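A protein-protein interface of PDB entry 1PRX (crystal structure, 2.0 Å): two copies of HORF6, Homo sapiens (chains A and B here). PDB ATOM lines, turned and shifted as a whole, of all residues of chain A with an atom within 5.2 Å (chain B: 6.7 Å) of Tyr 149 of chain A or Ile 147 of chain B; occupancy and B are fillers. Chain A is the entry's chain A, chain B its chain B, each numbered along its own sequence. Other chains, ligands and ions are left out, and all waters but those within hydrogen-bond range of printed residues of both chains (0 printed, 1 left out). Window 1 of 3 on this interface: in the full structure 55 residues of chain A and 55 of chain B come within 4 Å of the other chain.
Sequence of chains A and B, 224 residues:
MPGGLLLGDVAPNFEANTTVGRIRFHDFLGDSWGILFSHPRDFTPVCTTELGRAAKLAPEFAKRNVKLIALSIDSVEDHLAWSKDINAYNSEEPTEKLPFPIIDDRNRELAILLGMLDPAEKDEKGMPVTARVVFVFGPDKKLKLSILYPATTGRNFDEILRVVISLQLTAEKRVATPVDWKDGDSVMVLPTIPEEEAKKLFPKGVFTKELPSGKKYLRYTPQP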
ATOM      1  N   ARG A 132       7.257 -37.347 -23.843  1.00  0.00           N
ATOM      2  CA  ARG A 132       6.675 -36.530 -22.779  1.00  0.00           C
ATOM      3  C   ARG A 132       5.171 -36.336 -22.888  1.00  0.00           C
ATOM      4  O   ARG A 132       4.598 -35.506 -22.188  1.00  0.00           O
ATOM      5  CB  ARG A 132       7.352 -35.156 -22.780  1.00  0.00           C
ATOM      6  CG  ARG A 132       8.652 -35.125 -22.025  1.00  0.00           C
ATOM      7  CD  ARG A 132       8.382 -35.113 -20.541  1.00  0.00           C
ATOM      8  NE  ARG A 132       7.775 -33.848 -20.131  1.00  0.00           N
ATOM      9  CZ  ARG A 132       7.374 -33.564 -18.892  1.00  0.00           C
ATOM     10  NH1 ARG A 132       7.513 -34.468 -17.940  1.00  0.00           N
ATOM     11  NH2 ARG A 132       6.861 -32.369 -18.595  1.00  0.00           N
ATOM     12  N   SER A 146      -4.676 -34.686 -25.225  1.00  0.00           N
ATOM     13  CA  SER A 146      -3.257 -34.948 -24.997  1.00  0.00           C
ATOM     14  C   SER A 146      -2.529 -33.618 -24.809  1.00  0.00           C
ATOM     15  O   SER A 146      -2.986 -32.565 -25.260  1.00  0.00           O
ATOM     16  CB  SER A 146      -2.630 -35.799 -26.117  1.00  0.00           C
ATOM     17  OG  SER A 146      -2.514 -35.107 -27.345  1.00  0.00           O
ATOM     18  N   ILE A 147      -1.428 -33.667 -24.079  1.00  0.00           N
ATOM     19  CA  ILE A 147      -0.618 -32.485 -23.781  1.00  0.00           C
ATOM     20  C   ILE A 147       0.822 -32.903 -24.027  1.00  0.00           C
ATOM     21  O   ILE A 147       1.199 -34.026 -23.715  1.00  0.00           O
ATOM     22  CB  ILE A 147      -0.835 -32.071 -22.295  1.00  0.00           C
ATOM     23  CG1 ILE A 147      -2.244 -31.498 -22.126  1.00  0.00           C
ATOM     24  CG2 ILE A 147       0.198 -31.075 -21.842  1.00  0.00           C
ATOM     25  CD1 ILE A 147      -2.766 -31.523 -20.688  1.00  0.00           C
ATOM     26  N   LEU A 148       1.598 -32.049 -24.671  1.00  0.00           N
ATOM     27  CA  LEU A 148       2.988 -32.386 -24.948  1.00  0.00           C
ATOM     28  C   LEU A 148       3.904 -31.274 -24.452  1.00  0.00           C
ATOM     29  O   LEU A 148       4.203 -30.339 -25.189  1.00  0.00           O
ATOM     30  CB  LEU A 148       3.193 -32.596 -26.451  1.00  0.00           C
ATOM     31  CG  LEU A 148       4.222 -33.614 -26.959  1.00  0.00           C
ATOM     32  CD1 LEU A 148       4.755 -33.114 -28.302  1.00  0.00           C
ATOM     33  CD2 LEU A 148       5.373 -33.865 -25.968  1.00  0.00           C
ATOM     34  N   TYR A 149       4.307 -31.365 -23.190  1.00  0.00           N
ATOM     35  CA  TYR A 149       5.196 -30.384 -22.586  1.00  0.00           C
ATOM     36  C   TYR A 149       6.585 -30.999 -22.531  1.00  0.00           C
ATOM     37  O   TYR A 149       6.732 -32.187 -22.255  1.00  0.00           O
ATOM     38  CB  TYR A 149       4.767 -30.043 -21.151  1.00  0.00           C
ATOM     39  CG  TYR A 149       3.542 -29.160 -20.973  1.00  0.00           C
ATOM     40  CD1 TYR A 149       2.698 -28.834 -22.039  1.00  0.00           C
ATOM     41  CD2 TYR A 149       3.215 -28.680 -19.712  1.00  0.00           C
ATOM     42  CE1 TYR A 149       1.559 -28.054 -21.836  1.00  0.00           C
ATOM     43  CE2 TYR A 149       2.086 -27.908 -19.498  1.00  0.00           C
ATOM     44  CZ  TYR A 149       1.260 -27.598 -20.557  1.00  0.00           C
ATOM     45  OH  TYR A 149       0.128 -26.859 -20.316  1.00  0.00           O
ATOM     46  N   PRO A 150       7.626 -30.206 -22.829  1.00  0.00           N
ATOM     47  CA  PRO A 150       9.000 -30.708 -22.794  1.00  0.00           C
ATOM     48  C   PRO A 150       9.348 -31.071 -21.354  1.00  0.00           C
ATOM     49  O   PRO A 150       8.624 -30.691 -20.429  1.00  0.00           O
ATOM     50  CB  PRO A 150       9.806 -29.512 -23.304  1.00  0.00           C
ATOM     51  CG  PRO A 150       8.976 -28.346 -22.884  1.00  0.00           C
ATOM     52  CD  PRO A 150       7.594 -28.797 -23.249  1.00  0.00           C
ATOM     53  N   ALA A 151      10.475 -31.741 -21.147  1.00  0.00           N
ATOM     54  CA  ALA A 151      10.877 -32.191 -19.817  1.00  0.00           C
ATOM     55  C   ALA A 151      11.379 -31.071 -18.935  1.00  0.00           C
ATOM     56  O   ALA A 151      11.768 -31.318 -17.780  1.00  0.00           O
ATOM     57  CB  ALA A 151      11.953 -33.287 -19.936  1.00  0.00           C
ATOM     58  N   THR A 153       9.578 -28.142 -18.761  1.00  0.00           N
ATOM     59  CA  THR A 153       8.373 -27.402 -18.380  1.00  0.00           C
ATOM     60  C   THR A 153       7.415 -28.335 -17.659  1.00  0.00           C
ATOM     61  O   THR A 153       6.672 -29.092 -18.298  1.00  0.00           O
ATOM     62  CB  THR A 153       7.643 -26.796 -19.614  1.00  0.00           C
ATOM     63  OG1 THR A 153       8.471 -25.794 -20.199  1.00  0.00           O
ATOM     64  CG2 THR A 153       6.334 -26.139 -19.207  1.00  0.00           C
ATOM     65  N   GLY A 154       7.421 -28.259 -16.328  1.00  0.00           N
ATOM     66  CA  GLY A 154       6.556 -29.098 -15.521  1.00  0.00           C
ATOM     67  C   GLY A 154       5.083 -28.869 -15.794  1.00  0.00           C
ATOM     68  O   GLY A 154       4.651 -27.739 -16.015  1.00  0.00           O
ATOM     69  N   ARG A 155       4.309 -29.949 -15.786  1.00  0.00           N
ATOM     70  CA  ARG A 155       2.884 -29.844 -16.035  1.00  0.00           C
ATOM     71  C   ARG A 155       2.168 -29.116 -14.913  1.00  0.00           C
ATOM     72  O   ARG A 155       2.699 -28.958 -13.820  1.00  0.00           O
ATOM     73  CB  ARG A 155       2.266 -31.235 -16.228  1.00  0.00           C
ATOM     74  CG  ARG A 155       2.741 -31.936 -17.496  1.00  0.00           C
ATOM     75  CD  ARG A 155       3.046 -33.393 -17.196  1.00  0.00           C
ATOM     76  NE  ARG A 155       3.616 -34.119 -18.334  1.00  0.00           N
ATOM     77  CZ  ARG A 155       4.015 -35.390 -18.295  1.00  0.00           C
ATOM     78  NH1 ARG A 155       3.917 -36.078 -17.164  1.00  0.00           N
ATOM     79  NH2 ARG A 155       4.422 -35.992 -19.408  1.00  0.00           N
ATOM     80  N   ASN A 156       0.962 -28.662 -15.211  1.00  0.00           N
ATOM     81  CA  ASN A 156       0.102 -27.980 -14.260  1.00  0.00           C
ATOM     82  C   ASN A 156      -1.052 -28.956 -13.976  1.00  0.00           C
ATOM     83  O   ASN A 156      -1.859 -29.258 -14.861  1.00  0.00           O
ATOM     84  CB  ASN A 156      -0.415 -26.682 -14.895  1.00  0.00           C
ATOM     85  CG  ASN A 156      -1.497 -26.014 -14.078  1.00  0.00           C
ATOM     86  OD1 ASN A 156      -1.967 -26.551 -13.078  1.00  0.00           O
ATOM     87  ND2 ASN A 156      -1.935 -24.859 -14.532  1.00  0.00           N
ATOM     88  N   PRO B   2      -0.370 -36.130 -30.349  1.00  0.00           N
ATOM     89  CA  PRO B   2      -0.593 -34.699 -30.647  1.00  0.00           C
ATOM     90  C   PRO B   2      -0.562 -34.543 -32.170  1.00  0.00           C
ATOM     91  O   PRO B   2      -1.188 -35.347 -32.873  1.00  0.00           O
ATOM     92  CB  PRO B   2       0.558 -33.932 -30.004  1.00  0.00           C
ATOM     93  CG  PRO B   2       0.974 -34.892 -28.872  1.00  0.00           C
ATOM     94  CD  PRO B   2       0.827 -36.299 -29.515  1.00  0.00           C
ATOM     95  N   LEU B   7       8.739 -33.278 -30.531  1.00  0.00           N
ATOM     96  CA  LEU B   7       9.456 -32.153 -29.933  1.00  0.00           C
ATOM     97  C   LEU B   7      10.805 -32.121 -30.638  1.00  0.00           C
ATOM     98  O   LEU B   7      11.424 -33.161 -30.835  1.00  0.00           O
ATOM     99  CB  LEU B   7       9.673 -32.363 -28.423  1.00  0.00           C
ATOM    100  CG  LEU B   7       8.480 -32.312 -27.466  1.00  0.00           C
ATOM    101  CD1 LEU B   7       8.919 -32.523 -26.022  1.00  0.00           C
ATOM    102  CD2 LEU B   7       7.800 -30.971 -27.613  1.00  0.00           C
ATOM    103  N   ARG B 132      -7.253 -29.729 -34.005  1.00  0.00           N
ATOM    104  CA  ARG B 132      -7.333 -28.932 -32.791  1.00  0.00           C
ATOM    105  C   ARG B 132      -6.014 -28.629 -32.082  1.00  0.00           C
ATOM    106  O   ARG B 132      -6.012 -28.009 -31.034  1.00  0.00           O
ATOM    107  CB  ARG B 132      -8.300 -29.605 -31.810  1.00  0.00           C
ATOM    108  CG  ARG B 132      -9.754 -29.292 -32.070  1.00  0.00           C
ATOM    109  CD  ARG B 132     -10.101 -27.876 -31.628  1.00  0.00           C
ATOM    110  NE  ARG B 132      -9.918 -27.687 -30.178  1.00  0.00           N
ATOM    111  CZ  ARG B 132     -10.047 -26.518 -29.548  1.00  0.00           C
ATOM    112  NH1 ARG B 132     -10.366 -25.424 -30.235  1.00  0.00           N
ATOM    113  NH2 ARG B 132      -9.839 -26.431 -28.236  1.00  0.00           N
ATOM    114  N   VAL B 133      -4.896 -29.003 -32.686  1.00  0.00           N
ATOM    115  CA  VAL B 133      -3.589 -28.781 -32.070  1.00  0.00           C
ATOM    116  C   VAL B 133      -3.134 -27.321 -31.962  1.00  0.00           C
ATOM    117  O   VAL B 133      -3.414 -26.500 -32.843  1.00  0.00           O
ATOM    118  CB  VAL B 133      -2.490 -29.542 -32.831  1.00  0.00           C
ATOM    119  CG1 VAL B 133      -1.166 -29.399 -32.131  1.00  0.00           C
ATOM    120  CG2 VAL B 133      -2.857 -30.991 -32.979  1.00  0.00           C
ATOM    121  N   VAL B 134      -2.488 -26.997 -30.844  1.00  0.00           N
ATOM    122  CA  VAL B 134      -1.895 -25.680 -30.623  1.00  0.00           C
ATOM    123  C   VAL B 134      -0.402 -26.015 -30.664  1.00  0.00           C
ATOM    124  O   VAL B 134       0.076 -26.867 -29.903  1.00  0.00           O
ATOM    125  CB  VAL B 134      -2.248 -25.082 -29.246  1.00  0.00           C
ATOM    126  CG1 VAL B 134      -1.463 -23.807 -29.006  1.00  0.00           C
ATOM    127  CG2 VAL B 134      -3.698 -24.753 -29.182  1.00  0.00           C
ATOM    128  N   PHE B 135       0.314 -25.427 -31.612  1.00  0.00           N
ATOM    129  CA  PHE B 135       1.743 -25.683 -31.747  1.00  0.00           C
ATOM    130  C   PHE B 135       2.523 -24.454 -31.315  1.00  0.00           C
ATOM    131  O   PHE B 135       2.143 -23.328 -31.662  1.00  0.00           O
ATOM    132  CB  PHE B 135       2.122 -25.924 -33.212  1.00  0.00           C
ATOM    133  CG  PHE B 135       1.401 -27.064 -33.882  1.00  0.00           C
ATOM    134  CD1 PHE B 135       0.210 -26.842 -34.575  1.00  0.00           C
ATOM    135  CD2 PHE B 135       1.971 -28.334 -33.926  1.00  0.00           C
ATOM    136  CE1 PHE B 135      -0.395 -27.875 -35.311  1.00  0.00           C
ATOM    137  CE2 PHE B 135       1.375 -29.364 -34.658  1.00  0.00           C
ATOM    138  CZ  PHE B 135       0.196 -29.132 -35.350  1.00  0.00           C
ATOM    139  N   VAL B 136       3.621 -24.666 -30.594  1.00  0.00           N
ATOM    140  CA  VAL B 136       4.499 -23.558 -30.181  1.00  0.00           C
ATOM    141  C   VAL B 136       5.884 -23.822 -30.773  1.00  0.00           C
ATOM    142  O   VAL B 136       6.487 -24.860 -30.513  1.00  0.00           O
ATOM    143  CB  VAL B 136       4.637 -23.428 -28.635  1.00  0.00           C
ATOM    144  CG1 VAL B 136       5.501 -22.216 -28.280  1.00  0.00           C
ATOM    145  CG2 VAL B 136       3.276 -23.284 -27.991  1.00  0.00           C
ATOM    146  N   LYS B 144       8.387 -26.727 -29.835  1.00  0.00           N
ATOM    147  CA  LYS B 144       8.757 -26.662 -28.427  1.00  0.00           C
ATOM    148  C   LYS B 144       7.716 -27.238 -27.473  1.00  0.00           C
ATOM    149  O   LYS B 144       8.035 -27.779 -26.406  1.00  0.00           O
ATOM    150  CB  LYS B 144       9.001 -25.194 -28.058  1.00  0.00           C
ATOM    151  CG  LYS B 144      10.062 -24.487 -28.908  1.00  0.00           C
ATOM    152  CD  LYS B 144      11.473 -25.016 -28.617  1.00  0.00           C
ATOM    153  CE  LYS B 144      12.493 -24.452 -29.596  1.00  0.00           C
ATOM    154  NZ  LYS B 144      13.795 -25.172 -29.513  1.00  0.00           N
ATOM    155  N   LEU B 145       6.456 -27.105 -27.865  1.00  0.00           N
ATOM    156  CA  LEU B 145       5.335 -27.539 -27.036  1.00  0.00           C
ATOM    157  C   LEU B 145       4.137 -27.730 -27.956  1.00  0.00           C
ATOM    158  O   LEU B 145       4.037 -27.081 -29.005  1.00  0.00           O
ATOM    159  CB  LEU B 145       5.053 -26.409 -26.030  1.00  0.00           C
ATOM    160  CG  LEU B 145       4.102 -26.331 -24.823  1.00  0.00           C
ATOM    161  CD1 LEU B 145       2.758 -26.936 -25.091  1.00  0.00           C
ATOM    162  CD2 LEU B 145       4.751 -26.944 -23.635  1.00  0.00           C
ATOM    163  N   SER B 146       3.209 -28.576 -27.526  1.00  0.00           N
ATOM    164  CA  SER B 146       2.004 -28.887 -28.284  1.00  0.00           C
ATOM    165  C   SER B 146       0.883 -29.174 -27.274  1.00  0.00           C
ATOM    166  O   SER B 146       1.116 -29.774 -26.214  1.00  0.00           O
ATOM    167  CB  SER B 146       2.271 -30.125 -29.152  1.00  0.00           C
ATOM    168  OG  SER B 146       1.199 -30.419 -30.018  1.00  0.00           O
ATOM    169  N   ILE B 147      -0.337 -28.781 -27.620  1.00  0.00           N
ATOM    170  CA  ILE B 147      -1.504 -28.994 -26.753  1.00  0.00           C
ATOM    171  C   ILE B 147      -2.644 -29.466 -27.654  1.00  0.00           C
ATOM    172  O   ILE B 147      -2.842 -28.905 -28.733  1.00  0.00           O
ATOM    173  CB  ILE B 147      -1.862 -27.679 -26.001  1.00  0.00           C
ATOM    174  CG1 ILE B 147      -0.958 -27.492 -24.783  1.00  0.00           C
ATOM    175  CG2 ILE B 147      -3.319 -27.627 -25.608  1.00  0.00           C
ATOM    176  CD1 ILE B 147      -1.158 -26.152 -24.083  1.00  0.00           C
ATOM    177  N   LEU B 148      -3.324 -30.542 -27.261  1.00  0.00           N
ATOM    178  CA  LEU B 148      -4.420 -31.090 -28.071  1.00  0.00           C
ATOM    179  C   LEU B 148      -5.717 -31.251 -27.284  1.00  0.00           C
ATOM    180  O   LEU B 148      -6.008 -32.328 -26.760  1.00  0.00           O
ATOM    181  CB  LEU B 148      -4.038 -32.447 -28.703  1.00  0.00           C
ATOM    182  CG  LEU B 148      -4.498 -32.843 -30.130  1.00  0.00           C
ATOM    183  CD1 LEU B 148      -4.543 -34.341 -30.273  1.00  0.00           C
ATOM    184  CD2 LEU B 148      -5.826 -32.266 -30.476  1.00  0.00           C
ATOM    185  N   TYR B 149      -6.477 -30.164 -27.206  1.00  0.00           N
ATOM    186  CA  TYR B 149      -7.763 -30.144 -26.531  1.00  0.00           C
ATOM    187  C   TYR B 149      -8.839 -30.345 -27.585  1.00  0.00           C
ATOM    188  O   TYR B 149      -8.695 -29.903 -28.724  1.00  0.00           O
ATOM    189  CB  TYR B 149      -8.000 -28.779 -25.878  1.00  0.00           C
ATOM    190  CG  TYR B 149      -7.206 -28.526 -24.631  1.00  0.00           C
ATOM    191  CD1 TYR B 149      -6.093 -29.316 -24.316  1.00  0.00           C
ATOM    192  CD2 TYR B 149      -7.587 -27.533 -23.735  1.00  0.00           C
ATOM    193  CE1 TYR B 149      -5.390 -29.131 -23.140  1.00  0.00           C
ATOM    194  CE2 TYR B 149      -6.884 -27.335 -22.549  1.00  0.00           C
ATOM    195  CZ  TYR B 149      -5.789 -28.141 -22.258  1.00  0.00           C
ATOM    196  OH  TYR B 149      -5.106 -27.980 -21.082  1.00  0.00           O
ATOM    197  N   ARG B 155      -9.544 -23.997 -24.295  1.00  0.00           N
ATOM    198  CA  ARG B 155      -8.197 -23.869 -23.773  1.00  0.00           C
ATOM    199  C   ARG B 155      -8.160 -22.823 -22.668  1.00  0.00           C
ATOM    200  O   ARG B 155      -9.081 -22.023 -22.520  1.00  0.00           O
ATOM    201  CB  ARG B 155      -7.246 -23.475 -24.898  1.00  0.00           C
ATOM    202  CG  ARG B 155      -7.239 -24.460 -26.059  1.00  0.00           C
ATOM    203  CD  ARG B 155      -6.640 -23.821 -27.313  1.00  0.00           C
ATOM    204  NE  ARG B 155      -6.689 -24.734 -28.459  1.00  0.00           N
ATOM    205  CZ  ARG B 155      -6.899 -24.359 -29.720  1.00  0.00           C
ATOM    206  NH1 ARG B 155      -7.092 -23.075 -30.011  1.00  0.00           N
ATOM    207  NH2 ARG B 155      -6.865 -25.266 -30.687  1.00  0.00           N
ATOM    208  N   ASN B 156      -7.104 -22.875 -21.869  1.00  0.00           N
ATOM    209  CA  ASN B 156      -6.891 -21.952 -20.769  1.00  0.00           C
ATOM    210  C   ASN B 156      -5.702 -21.107 -21.202  1.00  0.00           C
ATOM    211  O   ASN B 156      -4.578 -21.606 -21.284  1.00  0.00           O
ATOM    212  CB  ASN B 156      -6.555 -22.758 -19.510  1.00  0.00           C
ATOM    213  CG  ASN B 156      -6.242 -21.884 -18.313  1.00  0.00           C
ATOM    214  OD1 ASN B 156      -6.059 -20.670 -18.431  1.00  0.00           O
ATOM    215  ND2 ASN B 156      -6.164 -22.503 -17.149  1.00  0.00           N
ATOM    216  N   GLU B 159      -2.660 -20.521 -18.893  1.00  0.00           N
ATOM    217  CA  GLU B 159      -1.771 -21.672 -18.925  1.00  0.00           C
ATOM    218  C   GLU B 159      -0.875 -21.567 -20.157  1.00  0.00           C
ATOM    219  O   GLU B 159       0.328 -21.850 -20.089  1.00  0.00           O
ATOM    220  CB  GLU B 159      -2.576 -22.972 -18.960  1.00  0.00           C
ATOM    221  CG  GLU B 159      -1.715 -24.231 -19.069  1.00  0.00           C
ATOM    222  CD  GLU B 159      -0.725 -24.393 -17.925  1.00  0.00           C
ATOM    223  OE1 GLU B 159      -0.826 -23.675 -16.911  1.00  0.00           O
ATOM    224  OE2 GLU B 159       0.169 -25.250 -18.025  1.00  0.00           O
ATOM    225  N   ILE B 160      -1.451 -21.124 -21.274  1.00  0.00           N
ATOM    226  CA  ILE B 160      -0.670 -20.961 -22.491  1.00  0.00           C
ATOM    227  C   ILE B 160       0.397 -19.875 -22.275  1.00  0.00           C
ATOM    228  O   ILE B 160       1.536 -20.021 -22.702  1.00  0.00           O
ATOM    229  CB  ILE B 160      -1.568 -20.638 -23.706  1.00  0.00           C
ATOM    230  CG1 ILE B 160      -2.373 -21.882 -24.102  1.00  0.00           C
ATOM    231  CG2 ILE B 160      -0.726 -20.154 -24.896  1.00  0.00           C
ATOM    232  CD1 ILE B 160      -3.368 -21.648 -25.260  1.00  0.00           C
ATOM    233  N   ARG B 162       1.637 -18.969 -19.273  1.00  0.00           N
ATOM    234  CA  ARG B 162       2.539 -19.520 -18.257  1.00  0.00           C
ATOM    235  C   ARG B 162       3.627 -20.422 -18.864  1.00  0.00           C
ATOM    236  O   ARG B 162       4.791 -20.369 -18.478  1.00  0.00           O
ATOM    237  CB  ARG B 162       1.700 -20.315 -17.249  1.00  0.00           C
ATOM    238  CG  ARG B 162       2.474 -21.027 -16.172  1.00  0.00           C
ATOM    239  CD  ARG B 162       1.651 -22.165 -15.590  1.00  0.00           C
ATOM    240  NE  ARG B 162       2.549 -23.145 -15.017  1.00  0.00           N
ATOM    241  CZ  ARG B 162       2.877 -24.306 -15.572  1.00  0.00           C
ATOM    242  NH1 ARG B 162       2.355 -24.695 -16.718  1.00  0.00           N
ATOM    243  NH2 ARG B 162       3.846 -25.021 -15.030  1.00  0.00           N
ATOM    244  N   VAL B 163       3.220 -21.256 -19.809  1.00  0.00           N
ATOM    245  CA  VAL B 163       4.079 -22.208 -20.493  1.00  0.00           C
ATOM    246  C   VAL B 163       5.089 -21.524 -21.428  1.00  0.00           C
ATOM    247  O   VAL B 163       6.210 -21.998 -21.592  1.00  0.00           O
ATOM    248  CB  VAL B 163       3.167 -23.277 -21.184  1.00  0.00           C
ATOM    249  CG1 VAL B 163       3.444 -23.430 -22.651  1.00  0.00           C
ATOM    250  CG2 VAL B 163       3.256 -24.581 -20.450  1.00  0.00           C
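The backbone carbonyl oxygen (O) of Tyr 149 of chain A is in hydrogen-bond range of the guanidinium group (NE) of Arg 132 of chain A (2.9 Å).
NH2 of Arg 132 of chain A is in hydrogen-bond range of O of Thr 153 of chain A (3.3 Å).
The backbone carbonyl oxygen (O) of Ile 147 of chain B is in hydrogen-bond range of the backbone NH (N) of Val 134 of chain B, 2.9 Å away.
O of Val 136 of chain B is in hydrogen-bond range of N of Lys 144 of chain B (2.7 Å).
The backbone NH (N) of Glu 159 of chain B is in hydrogen-bond range of the side-chain amide oxygen (OD1) of Asn 156 of chain B (3.4 Å).
The guanidinium group (NH1) of Arg 162 of chain B is in salt-bridge range of the side-chain carboxylate (OE2) of Glu 159 of chain B, 2.6 Å away.
Hydrophobic or aromatic side chains of chain B within 4 Å of the printed part of chain A: Pro 2, Leu 7, Leu 145, Ile 147, Leu 148 and Val 163.
Hydrophobic or aromatic side chains of chain A within 4 Å of the printed part of chain B: Leu 148, Tyr 149 and Pro 150.
Among the printed residues, 19 pairs touch across the chains.
Among the printed residues, no Asp or Glu carboxylate lies within 4 Å of a Lys or Arg side-chain nitrogen of the other chain.
Printed residues of chain B within 4 Å of Tyr 149 of chain A: Leu 145 (3.2 Å), Ile 147 (3.9 Å), Glu 159 (2.8 Å) and Val 163 (3.6 Å).
Of chain A, only Ser 146 (3.9 Å) and Tyr 149 (3.9 Å) come within 4 Å of Ile 147 of chain B.
Of the printed residues of chain A, Lys 144 of chain B touches Pro 150 (3.3 Å).
Of the printed residues of chain B, Gly 154 of chain A touches Arg 162 (3.0 Å).
Ile 160 of chain B touches none of the printed residues of chain A.
Arg 132 of chain B touches none of the printed residues of chain A.
The nearest residue of chain B that does not touch Tyr 149 of chain A is Arg 162 of chain B (4.3 Å).
The nearest printed residue of chain A that does not touch Glu 159 of chain B is Arg 155 of chain A (5.4 Å).
Ser 146 of chain A touches Ile 147 of chain B, and with the chains exchanged Ile 147 of chain A touches Ser 146 of chain B.
Ser 146 of chain A touches Leu 148 of chain B, and with the chains exchanged Leu 148 of chain A touches Ser 146 of chain B.
Tyr 149 of chain A touches Ile 147 of chain B, but with the chains exchanged Ile 147 of chain A does not touch Tyr 149 of chain B (4.1 Å).
Of the 19 pairs that touch across the chains among the printed residues, 4 have their exchanged pair printed and touching as well.
Among the printed residues, merely in contact across the chains: Tyr 149 of chain A with Leu 145 of chain B (3.2 Å), Pro 150 of chain A with Lys 144 of chain B (3.3 Å), Pro 150 of chain A with Leu 145 of chain B (3.4 Å), Leu 148 of chain A with Leu 145 of chain B (3.5 Å), Tyr 149 of chain A with Val 163 of chain B (3.6 Å), Thr 153 of chain A with Val 163 of chain B (3.7 Å), Pro 150 of chain A with Leu 7 of chain B (3.7 Å), Leu 148 of chain A with Leu 7 of chain B (3.8 Å), Ser 146 of chain A with Pro 2 of chain B (3.8 Å), Ile 147 of chain A with Ser 146 of chain B (3.8 Å), Asn 156 of chain A with Arg 162 of chain B (3.9 Å), Tyr 149 of chain A with Ile 147 of chain B (3.9 Å), Ser 146 of chain A with Ile 147 of chain B (3.9 Å) and Leu 148 of chain A with Pro 2 of chain B (3.98 Å).
The backbone NH of Leu 148 of chain B is in hydrogen-bond range of the backbone carbonyl oxygen of Ser 146 of chain A (2.9 Å).
The backbone NH (N) of Leu 148 of chain A sits at hydrogen-bond distance from the backbone carbonyl oxygen (O) of Ser 146 of chain B.
OH of Tyr 149 of chain A sits at hydrogen-bond distance from OE2 of Glu 159 of chain B, at 2.8 Å.
O of Gly 154 of chain A lies within hydrogen-bond range of NH2 of Arg 162 of chain B.
The side-chain carboxylate (OE1) of Glu 159 of chain B is in hydrogen-bond range of the side-chain amide nitrogen (ND2) of Asn 156 of chain A (2.9 Å).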
